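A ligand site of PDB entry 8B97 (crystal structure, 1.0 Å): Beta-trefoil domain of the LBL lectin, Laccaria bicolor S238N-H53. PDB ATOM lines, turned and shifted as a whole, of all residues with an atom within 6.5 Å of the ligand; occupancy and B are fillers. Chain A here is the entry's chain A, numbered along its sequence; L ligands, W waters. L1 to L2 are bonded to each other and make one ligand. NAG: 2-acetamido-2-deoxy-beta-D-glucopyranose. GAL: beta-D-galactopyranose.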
ATOM      1  N   ARG A  22      34.030  10.244  -4.906  1.00  0.00           N
ATOM      2  CA  ARG A  22      33.145  11.374  -4.687  1.00  0.00           C
ATOM      3  C   ARG A  22      32.268  11.113  -3.467  1.00  0.00           C
ATOM      4  O   ARG A  22      31.907   9.972  -3.178  1.00  0.00           O
ATOM      5  CB  ARG A  22      32.297  11.661  -5.920  1.00  0.00           C
ATOM      6  CG  ARG A  22      33.151  12.043  -7.125  1.00  0.00           C
ATOM      7  CD  ARG A  22      32.361  12.286  -8.362  1.00  0.00           C
ATOM      8  NE  ARG A  22      33.216  12.655  -9.481  1.00  0.00           N
ATOM      9  CZ  ARG A  22      32.813  13.043 -10.669  1.00  0.00           C
ATOM     10  NH1 ARG A  22      31.537  13.299 -10.914  1.00  0.00           N
ATOM     11  NH2 ARG A  22      33.688  13.091 -11.672  1.00  0.00           N
ATOM     12  N   VAL A  23      31.933  12.209  -2.784  1.00  0.00           N
ATOM     13  CA  VAL A  23      31.125  12.157  -1.567  1.00  0.00           C
ATOM     14  C   VAL A  23      29.696  12.591  -1.883  1.00  0.00           C
ATOM     15  O   VAL A  23      29.466  13.522  -2.656  1.00  0.00           O
ATOM     16  CB  VAL A  23      31.719  13.011  -0.436  1.00  0.00           C
ATOM     17  CG1 VAL A  23      33.033  12.421   0.056  1.00  0.00           C
ATOM     18  CG2 VAL A  23      31.885  14.479  -0.845  1.00  0.00           C
ATOM     19  N   LEU A  24      28.743  11.932  -1.248  1.00  0.00           N
ATOM     20  CA  LEU A  24      27.342  12.290  -1.412  1.00  0.00           C
ATOM     21  C   LEU A  24      27.077  13.660  -0.806  1.00  0.00           C
ATOM     22  O   LEU A  24      27.772  14.113   0.108  1.00  0.00           O
ATOM     23  CB  LEU A  24      26.454  11.255  -0.728  1.00  0.00           C
ATOM     24  CG  LEU A  24      26.572   9.813  -1.233  1.00  0.00           C
ATOM     25  CD1 LEU A  24      25.622   8.904  -0.463  1.00  0.00           C
ATOM     26  CD2 LEU A  24      26.305   9.731  -2.718  1.00  0.00           C
ATOM     27  N   PHE A  25      26.026  14.329  -1.288  1.00  0.00           N
ATOM     28  CA  PHE A  25      25.611  15.573  -0.675  1.00  0.00           C
ATOM     29  C   PHE A  25      24.106  15.767  -0.773  1.00  0.00           C
ATOM     30  O   PHE A  25      23.427  15.154  -1.602  1.00  0.00           O
ATOM     31  CB  PHE A  25      26.376  16.782  -1.237  1.00  0.00           C
ATOM     32  CG  PHE A  25      26.068  17.135  -2.668  1.00  0.00           C
ATOM     33  CD1 PHE A  25      24.895  17.800  -3.018  1.00  0.00           C
ATOM     34  CD2 PHE A  25      27.012  16.903  -3.656  1.00  0.00           C
ATOM     35  CE1 PHE A  25      24.674  18.192  -4.341  1.00  0.00           C
ATOM     36  CE2 PHE A  25      26.791  17.290  -4.966  1.00  0.00           C
ATOM     37  CZ  PHE A  25      25.624  17.944  -5.298  1.00  0.00           C
ATOM     38  N   ARG A  27      21.583  19.301  -0.585  1.00  0.00           N
ATOM     39  CA  ARG A  27      21.493  20.755  -0.536  1.00  0.00           C
ATOM     40  C   ARG A  27      20.129  21.151  -1.087  1.00  0.00           C
ATOM     41  O   ARG A  27      19.494  20.406  -1.823  1.00  0.00           O
ATOM     42  CB  ARG A  27      22.618  21.421  -1.335  1.00  0.00           C
ATOM     43  CG  ARG A  27      22.584  21.159  -2.821  1.00  0.00           C
ATOM     44  CD  ARG A  27      23.862  21.598  -3.536  1.00  0.00           C
ATOM     45  NE  ARG A  27      23.685  21.406  -4.967  1.00  0.00           N
ATOM     46  CZ  ARG A  27      24.666  21.229  -5.831  1.00  0.00           C
ATOM     47  NH1 ARG A  27      25.932  21.445  -5.513  1.00  0.00           N
ATOM     48  NH2 ARG A  27      24.368  20.822  -7.063  1.00  0.00           N
ATOM     49  N   SER A  29      19.774  23.952  -2.932  1.00  0.00           N
ATOM     50  CA  SER A  29      20.059  24.623  -4.185  1.00  0.00           C
ATOM     51  C   SER A  29      21.565  24.592  -4.374  1.00  0.00           C
ATOM     52  O   SER A  29      22.309  24.507  -3.402  1.00  0.00           O
ATOM     53  CB  SER A  29      19.575  26.077  -4.155  1.00  0.00           C
ATOM     54  OG  SER A  29      20.398  26.896  -3.334  1.00  0.00           O
ATOM     55  N   PRO A  30      22.040  24.671  -5.618  1.00  0.00           N
ATOM     56  CA  PRO A  30      21.272  24.556  -6.857  1.00  0.00           C
ATOM     57  C   PRO A  30      20.907  23.093  -7.121  1.00  0.00           C
ATOM     58  O   PRO A  30      21.258  22.203  -6.361  1.00  0.00           O
ATOM     59  CB  PRO A  30      22.269  25.066  -7.910  1.00  0.00           C
ATOM     60  CG  PRO A  30      23.596  24.665  -7.366  1.00  0.00           C
ATOM     61  CD  PRO A  30      23.479  24.845  -5.873  1.00  0.00           C
ATOM     62  N   SER A  31      20.207  22.865  -8.224  1.00  0.00           N
ATOM     63  CA  SER A  31      19.984  21.513  -8.695  1.00  0.00           C
ATOM     64  C   SER A  31      21.271  20.957  -9.305  1.00  0.00           C
ATOM     65  O   SER A  31      22.010  21.695  -9.961  1.00  0.00           O
ATOM     66  CB  SER A  31      18.883  21.536  -9.756  1.00  0.00           C
ATOM     67  OG  SER A  31      18.662  20.268 -10.317  1.00  0.00           O
ATOM     68  N   PRO A  32      21.574  19.652  -9.122  1.00  0.00           N
ATOM     69  CA  PRO A  32      20.788  18.669  -8.371  1.00  0.00           C
ATOM     70  C   PRO A  32      20.949  18.826  -6.869  1.00  0.00           C
ATOM     71  O   PRO A  32      22.037  19.154  -6.374  1.00  0.00           O
ATOM     72  CB  PRO A  32      21.388  17.333  -8.823  1.00  0.00           C
ATOM     73  CG  PRO A  32      22.808  17.659  -9.127  1.00  0.00           C
ATOM     74  CD  PRO A  32      22.746  19.033  -9.756  1.00  0.00           C
ATOM     75  N   PHE A  35      23.404  14.549  -4.975  1.00  0.00           N
ATOM     76  CA  PHE A  35      24.367  14.148  -6.002  1.00  0.00           C
ATOM     77  C   PHE A  35      25.667  13.831  -5.260  1.00  0.00           C
ATOM     78  O   PHE A  35      25.638  13.463  -4.082  1.00  0.00           O
ATOM     79  CB  PHE A  35      24.400  15.244  -7.082  1.00  0.00           C
ATOM     80  CG  PHE A  35      25.251  14.934  -8.312  1.00  0.00           C
ATOM     81  CD1 PHE A  35      25.036  13.809  -9.070  1.00  0.00           C
ATOM     82  CD2 PHE A  35      26.253  15.811  -8.682  1.00  0.00           C
ATOM     83  CE1 PHE A  35      25.830  13.568 -10.197  1.00  0.00           C
ATOM     84  CE2 PHE A  35      27.040  15.583  -9.781  1.00  0.00           C
ATOM     85  CZ  PHE A  35      26.832  14.465 -10.537  1.00  0.00           C
ATOM     86  N   HIS A  36      26.796  13.931  -5.949  1.00  0.00           N
ATOM     87  CA  HIS A  36      28.075  13.644  -5.331  1.00  0.00           C
ATOM     88  C   HIS A  36      29.118  14.631  -5.859  1.00  0.00           C
ATOM     89  O   HIS A  36      28.917  15.303  -6.879  1.00  0.00           O
ATOM     90  CB  HIS A  36      28.511  12.179  -5.491  1.00  0.00           C
ATOM     91  CG  HIS A  36      28.697  11.711  -6.896  1.00  0.00           C
ATOM     92  ND1 HIS A  36      28.990  10.400  -7.174  1.00  0.00           N
ATOM     93  CD2 HIS A  36      28.611  12.359  -8.080  1.00  0.00           C
ATOM     94  CE1 HIS A  36      29.083  10.258  -8.480  1.00  0.00           C
ATOM     95  NE2 HIS A  36      28.858  11.434  -9.067  1.00  0.00           N
ATOM     96  N   HIS A  37      30.239  14.738  -5.137  1.00  0.00           N
ATOM     97  CA  HIS A  37      31.226  15.769  -5.390  1.00  0.00           C
ATOM     98  C   HIS A  37      32.628  15.224  -5.143  1.00  0.00           C
ATOM     99  O   HIS A  37      32.824  14.476  -4.189  1.00  0.00           O
ATOM    100  CB  HIS A  37      30.982  16.978  -4.474  1.00  0.00           C
ATOM    101  CG  HIS A  37      31.728  18.188  -4.930  1.00  0.00           C
ATOM    102  ND1 HIS A  37      31.315  18.912  -6.033  1.00  0.00           N
ATOM    103  CD2 HIS A  37      32.892  18.735  -4.494  1.00  0.00           C
ATOM    104  CE1 HIS A  37      32.203  19.869  -6.241  1.00  0.00           C
ATOM    105  NE2 HIS A  37      33.152  19.785  -5.331  1.00  0.00           N
ATOM    106  N   PRO A  38      33.624  15.624  -5.934  1.00  0.00           N
ATOM    107  CA  PRO A  38      34.995  15.150  -5.675  1.00  0.00           C
ATOM    108  C   PRO A  38      35.416  15.366  -4.232  1.00  0.00           C
ATOM    109  O   PRO A  38      35.273  16.447  -3.661  1.00  0.00           O
ATOM    110  CB  PRO A  38      35.824  15.979  -6.679  1.00  0.00           C
ATOM    111  CG  PRO A  38      34.887  16.154  -7.828  1.00  0.00           C
ATOM    112  CD  PRO A  38      33.548  16.422  -7.162  1.00  0.00           C
ATOM    113  N   GLU A  41      37.273  18.441  -2.252  1.00  0.00           N
ATOM    114  CA  GLU A  41      36.626  19.707  -1.935  1.00  0.00           C
ATOM    115  C   GLU A  41      35.538  19.443  -0.902  1.00  0.00           C
ATOM    116  O   GLU A  41      34.538  18.802  -1.199  1.00  0.00           O
ATOM    117  CB  GLU A  41      36.043  20.358  -3.185  1.00  0.00           C
ATOM    118  CG  GLU A  41      37.093  20.696  -4.235  1.00  0.00           C
ATOM    119  CD  GLU A  41      36.556  21.573  -5.329  1.00  0.00           C
ATOM    120  OE1 GLU A  41      35.332  21.506  -5.603  1.00  0.00           O
ATOM    121  OE2 GLU A  41      37.352  22.313  -5.942  1.00  0.00           O
ATOM    122  N   VAL A  42      35.747  19.950   0.303  1.00  0.00           N
ATOM    123  CA  VAL A  42      34.831  19.733   1.420  1.00  0.00           C
ATOM    124  C   VAL A  42      33.864  20.898   1.467  1.00  0.00           C
ATOM    125  O   VAL A  42      34.290  22.063   1.454  1.00  0.00           O
ATOM    126  CB  VAL A  42      35.605  19.610   2.746  1.00  0.00           C
ATOM    127  CG1 VAL A  42      34.653  19.291   3.881  1.00  0.00           C
ATOM    128  CG2 VAL A  42      36.693  18.558   2.644  1.00  0.00           C
ATOM    129  N   TYR A  43      32.579  20.592   1.500  1.00  0.00           N
ATOM    130  CA  TYR A  43      31.519  21.588   1.550  1.00  0.00           C
ATOM    131  C   TYR A  43      30.458  21.161   2.546  1.00  0.00           C
ATOM    132  O   TYR A  43      30.276  19.974   2.817  1.00  0.00           O
ATOM    133  CB  TYR A  43      30.857  21.789   0.172  1.00  0.00           C
ATOM    134  CG  TYR A  43      31.715  22.567  -0.815  1.00  0.00           C
ATOM    135  CD1 TYR A  43      31.940  23.917  -0.623  1.00  0.00           C
ATOM    136  CD2 TYR A  43      32.274  21.959  -1.920  1.00  0.00           C
ATOM    137  CE1 TYR A  43      32.703  24.640  -1.497  1.00  0.00           C
ATOM    138  CE2 TYR A  43      33.046  22.683  -2.824  1.00  0.00           C
ATOM    139  CZ  TYR A  43      33.262  24.032  -2.602  1.00  0.00           C
ATOM    140  OH  TYR A  43      34.011  24.781  -3.466  1.00  0.00           O
ATOM    141  N   PRO A  44      29.724  22.134   3.099  1.00  0.00           N
ATOM    142  CA  PRO A  44      28.738  21.833   4.151  1.00  0.00           C
ATOM    143  C   PRO A  44      27.710  20.775   3.780  1.00  0.00           C
ATOM    144  O   PRO A  44      27.293  19.980   4.641  1.00  0.00           O
ATOM    145  CB  PRO A  44      28.080  23.189   4.403  1.00  0.00           C
ATOM    146  CG  PRO A  44      29.175  24.156   4.144  1.00  0.00           C
ATOM    147  CD  PRO A  44      29.975  23.578   3.000  1.00  0.00           C
ATOM    148  N   ASP A  45      27.308  20.744   2.524  1.00  0.00           N
ATOM    149  CA  ASP A  45      26.269  19.821   2.089  1.00  0.00           C
ATOM    150  C   ASP A  45      26.703  18.365   2.090  1.00  0.00           C
ATOM    151  O   ASP A  45      25.854  17.488   1.866  1.00  0.00           O
ATOM    152  CB  ASP A  45      25.677  20.260   0.748  1.00  0.00           C
ATOM    153  CG  ASP A  45      26.703  20.486  -0.334  1.00  0.00           C
ATOM    154  OD1 ASP A  45      27.783  19.842  -0.310  1.00  0.00           O
ATOM    155  OD2 ASP A  45      26.393  21.302  -1.228  1.00  0.00           O
ATOM    156  N   GLN A  46      27.952  18.074   2.399  1.00  0.00           N
ATOM    157  CA  GLN A  46      28.455  16.700   2.382  1.00  0.00           C
ATOM    158  C   GLN A  46      28.387  16.008   3.738  1.00  0.00           C
ATOM    159  O   GLN A  46      28.790  14.844   3.847  1.00  0.00           O
ATOM    160  CB  GLN A  46      29.903  16.720   1.891  1.00  0.00           C
ATOM    161  CG  GLN A  46      30.025  17.321   0.506  1.00  0.00           C
ATOM    162  CD  GLN A  46      31.458  17.689   0.164  1.00  0.00           C
ATOM    163  OE1 GLN A  46      32.353  17.485   0.981  1.00  0.00           O
ATOM    164  NE2 GLN A  46      31.680  18.229  -1.021  1.00  0.00           N
ATOM    165  N   THR A 128      26.042  12.383 -15.762  1.00  0.00           N
ATOM    166  CA  THR A 128      25.757  12.853 -14.412  1.00  0.00           C
ATOM    167  C   THR A 128      24.307  12.609 -13.994  1.00  0.00           C
ATOM    168  O   THR A 128      24.060  12.473 -12.796  1.00  0.00           O
ATOM    169  CB  THR A 128      26.134  14.324 -14.213  1.00  0.00           C
ATOM    170  OG1 THR A 128      25.465  15.133 -15.175  1.00  0.00           O
ATOM    171  CG2 THR A 128      27.641  14.521 -14.342  1.00  0.00           C
ATOM    172  N   GLN A 131      24.668   9.124 -12.277  1.00  0.00           N
ATOM    173  CA  GLN A 131      25.864   8.759 -11.510  1.00  0.00           C
ATOM    174  C   GLN A 131      25.557   8.427 -10.050  1.00  0.00           C
ATOM    175  O   GLN A 131      26.322   7.671  -9.434  1.00  0.00           O
ATOM    176  CB  GLN A 131      26.871   9.909 -11.549  1.00  0.00           C
ATOM    177  CG  GLN A 131      27.635   9.958 -12.847  1.00  0.00           C
ATOM    178  CD  GLN A 131      28.674  11.045 -12.888  1.00  0.00           C
ATOM    179  OE1 GLN A 131      28.886  11.788 -11.929  1.00  0.00           O
ATOM    180  NE2 GLN A 131      29.350  11.149 -14.027  1.00  0.00           N
HETATM  181  C1  NAG L   1      28.847  21.107 -11.248  1.00  0.00           C
HETATM  182  C2  NAG L   1      28.098  20.230 -10.257  1.00  0.00           C
HETATM  183  C3  NAG L   1      27.731  21.013  -8.985  1.00  0.00           C
HETATM  184  C4  NAG L   1      28.985  21.690  -8.416  1.00  0.00           C
HETATM  185  C5  NAG L   1      29.653  22.501  -9.540  1.00  0.00           C
HETATM  186  C6  NAG L   1      30.932  23.161  -9.046  1.00  0.00           C
HETATM  187  C7  NAG L   1      26.898  18.584 -11.699  1.00  0.00           C
HETATM  188  C8  NAG L   1      25.577  18.114 -12.287  1.00  0.00           C
HETATM  189  N2  NAG L   1      26.868  19.741 -10.849  1.00  0.00           N
HETATM  190  O1  NAG L   1      27.979  22.103 -11.689  1.00  0.00           O
HETATM  191  O3  NAG L   1      27.137  20.178  -8.024  1.00  0.00           O
HETATM  192  O4  NAG L   1      28.569  22.556  -7.390  1.00  0.00           O
HETATM  193  O5  NAG L   1      29.967  21.671 -10.631  1.00  0.00           O
HETATM  194  O6  NAG L   1      31.833  22.200  -8.549  1.00  0.00           O
HETATM  195  O7  NAG L   1      27.906  18.018 -11.922  1.00  0.00           O
HETATM  196  C1  GAL L   2      29.277  22.463  -6.178  1.00  0.00           C
HETATM  197  C2  GAL L   2      28.958  23.734  -5.401  1.00  0.00           C
HETATM  198  C3  GAL L   2      29.507  23.619  -3.979  1.00  0.00           C
HETATM  199  C4  GAL L   2      28.917  22.378  -3.323  1.00  0.00           C
HETATM  200  C5  GAL L   2      29.333  21.182  -4.183  1.00  0.00           C
HETATM  201  C6  GAL L   2      28.796  19.862  -3.641  1.00  0.00           C
HETATM  202  O2  GAL L   2      29.488  24.854  -6.083  1.00  0.00           O
HETATM  203  O3  GAL L   2      29.174  24.769  -3.238  1.00  0.00           O
HETATM  204  O4  GAL L   2      27.530  22.498  -3.243  1.00  0.00           O
HETATM  205  O5  GAL L   2      28.816  21.328  -5.490  1.00  0.00           O
HETATM  206  O6  GAL L   2      29.418  19.519  -2.425  1.00  0.00           O
HETATM  207  O   HOH W   1      26.961  20.397 -14.606  1.00  0.00           O
HETATM  208  O   HOH W   2      31.805  19.811 -10.978  1.00  0.00           O
HETATM  209  O   HOH W   3      31.141  26.710  -3.894  1.00  0.00           O
HETATM  210  O   HOH W   4      29.240  18.015 -14.449  1.00  0.00           O
HETATM  211  O   HOH W   5      27.592  25.425  -8.262  1.00  0.00           O
HETATM  212  O   HOH W   6      32.062  25.366  -6.450  1.00  0.00           O
HETATM  213  O   HOH W   7      24.701  21.774 -10.634  1.00  0.00           O
HETATM  214  O   HOH W   8      26.624  25.146 -12.720  1.00  0.00           O
HETATM  215  O   HOH W   9      29.065  18.249  -7.603  1.00  0.00           O
HETATM  216  O   HOH W  10      28.705  24.808  -0.521  1.00  0.00           O
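An oxygen (O4) of GAL L2 sits at hydrogen-bond distance from the side-chain carboxylate of Asp 45 (2.6 Å). An oxygen (O6) of GAL L2 is in hydrogen-bond range of the side-chain amide nitrogen (NE2) of Gln 46. The guanidinium group (NH1) of Arg 27 lies within hydrogen-bond range of an oxygen (O5) of GAL L2 (2.9 Å).
The backbone NH (N) of Tyr 43 lies within hydrogen-bond range of the side-chain amide oxygen (OE1) of Gln 46 (3.2 Å). NE2 of Gln 46 lies within hydrogen-bond range of O of Glu 41. The backbone NH (N) of Val 23 is in hydrogen-bond range of the backbone carbonyl oxygen (O) of His 37, 2.8 Å away. O of Phe 35 sits at hydrogen-bond distance from N of Phe 25. The backbone carbonyl oxygen of Pro 32 sits at hydrogen-bond distance from the guanidinium group of Arg 27. The guanidinium group (NE) of Arg 27 sits at hydrogen-bond distance from the backbone carbonyl oxygen (O) of Pro 30, at 2.9 Å. OE1 of Glu 41 lies within hydrogen-bond range of NE2 of His 37 (2.8 Å).
Merely in contact with the ligand: His 37, Phe 35, Phe 25, Tyr 43 and Pro 32. Within 4 Å of the ligand: Phe 25, Arg 27, Pro 32, Phe 35, His 37, Tyr 43, Asp 45 and Gln 46.
Water W9 lies within hydrogen-bond range of O3 of NAG L1, ND1 of His 37 and O of His 36. Water W3 lies within hydrogen-bond range of O3 of GAL L2 and OH of Tyr 43. Water W7 lies within hydrogen-bond range of the backbone carbonyl oxygen of Ser 31 and a nitrogen (N2) of NAG L1.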
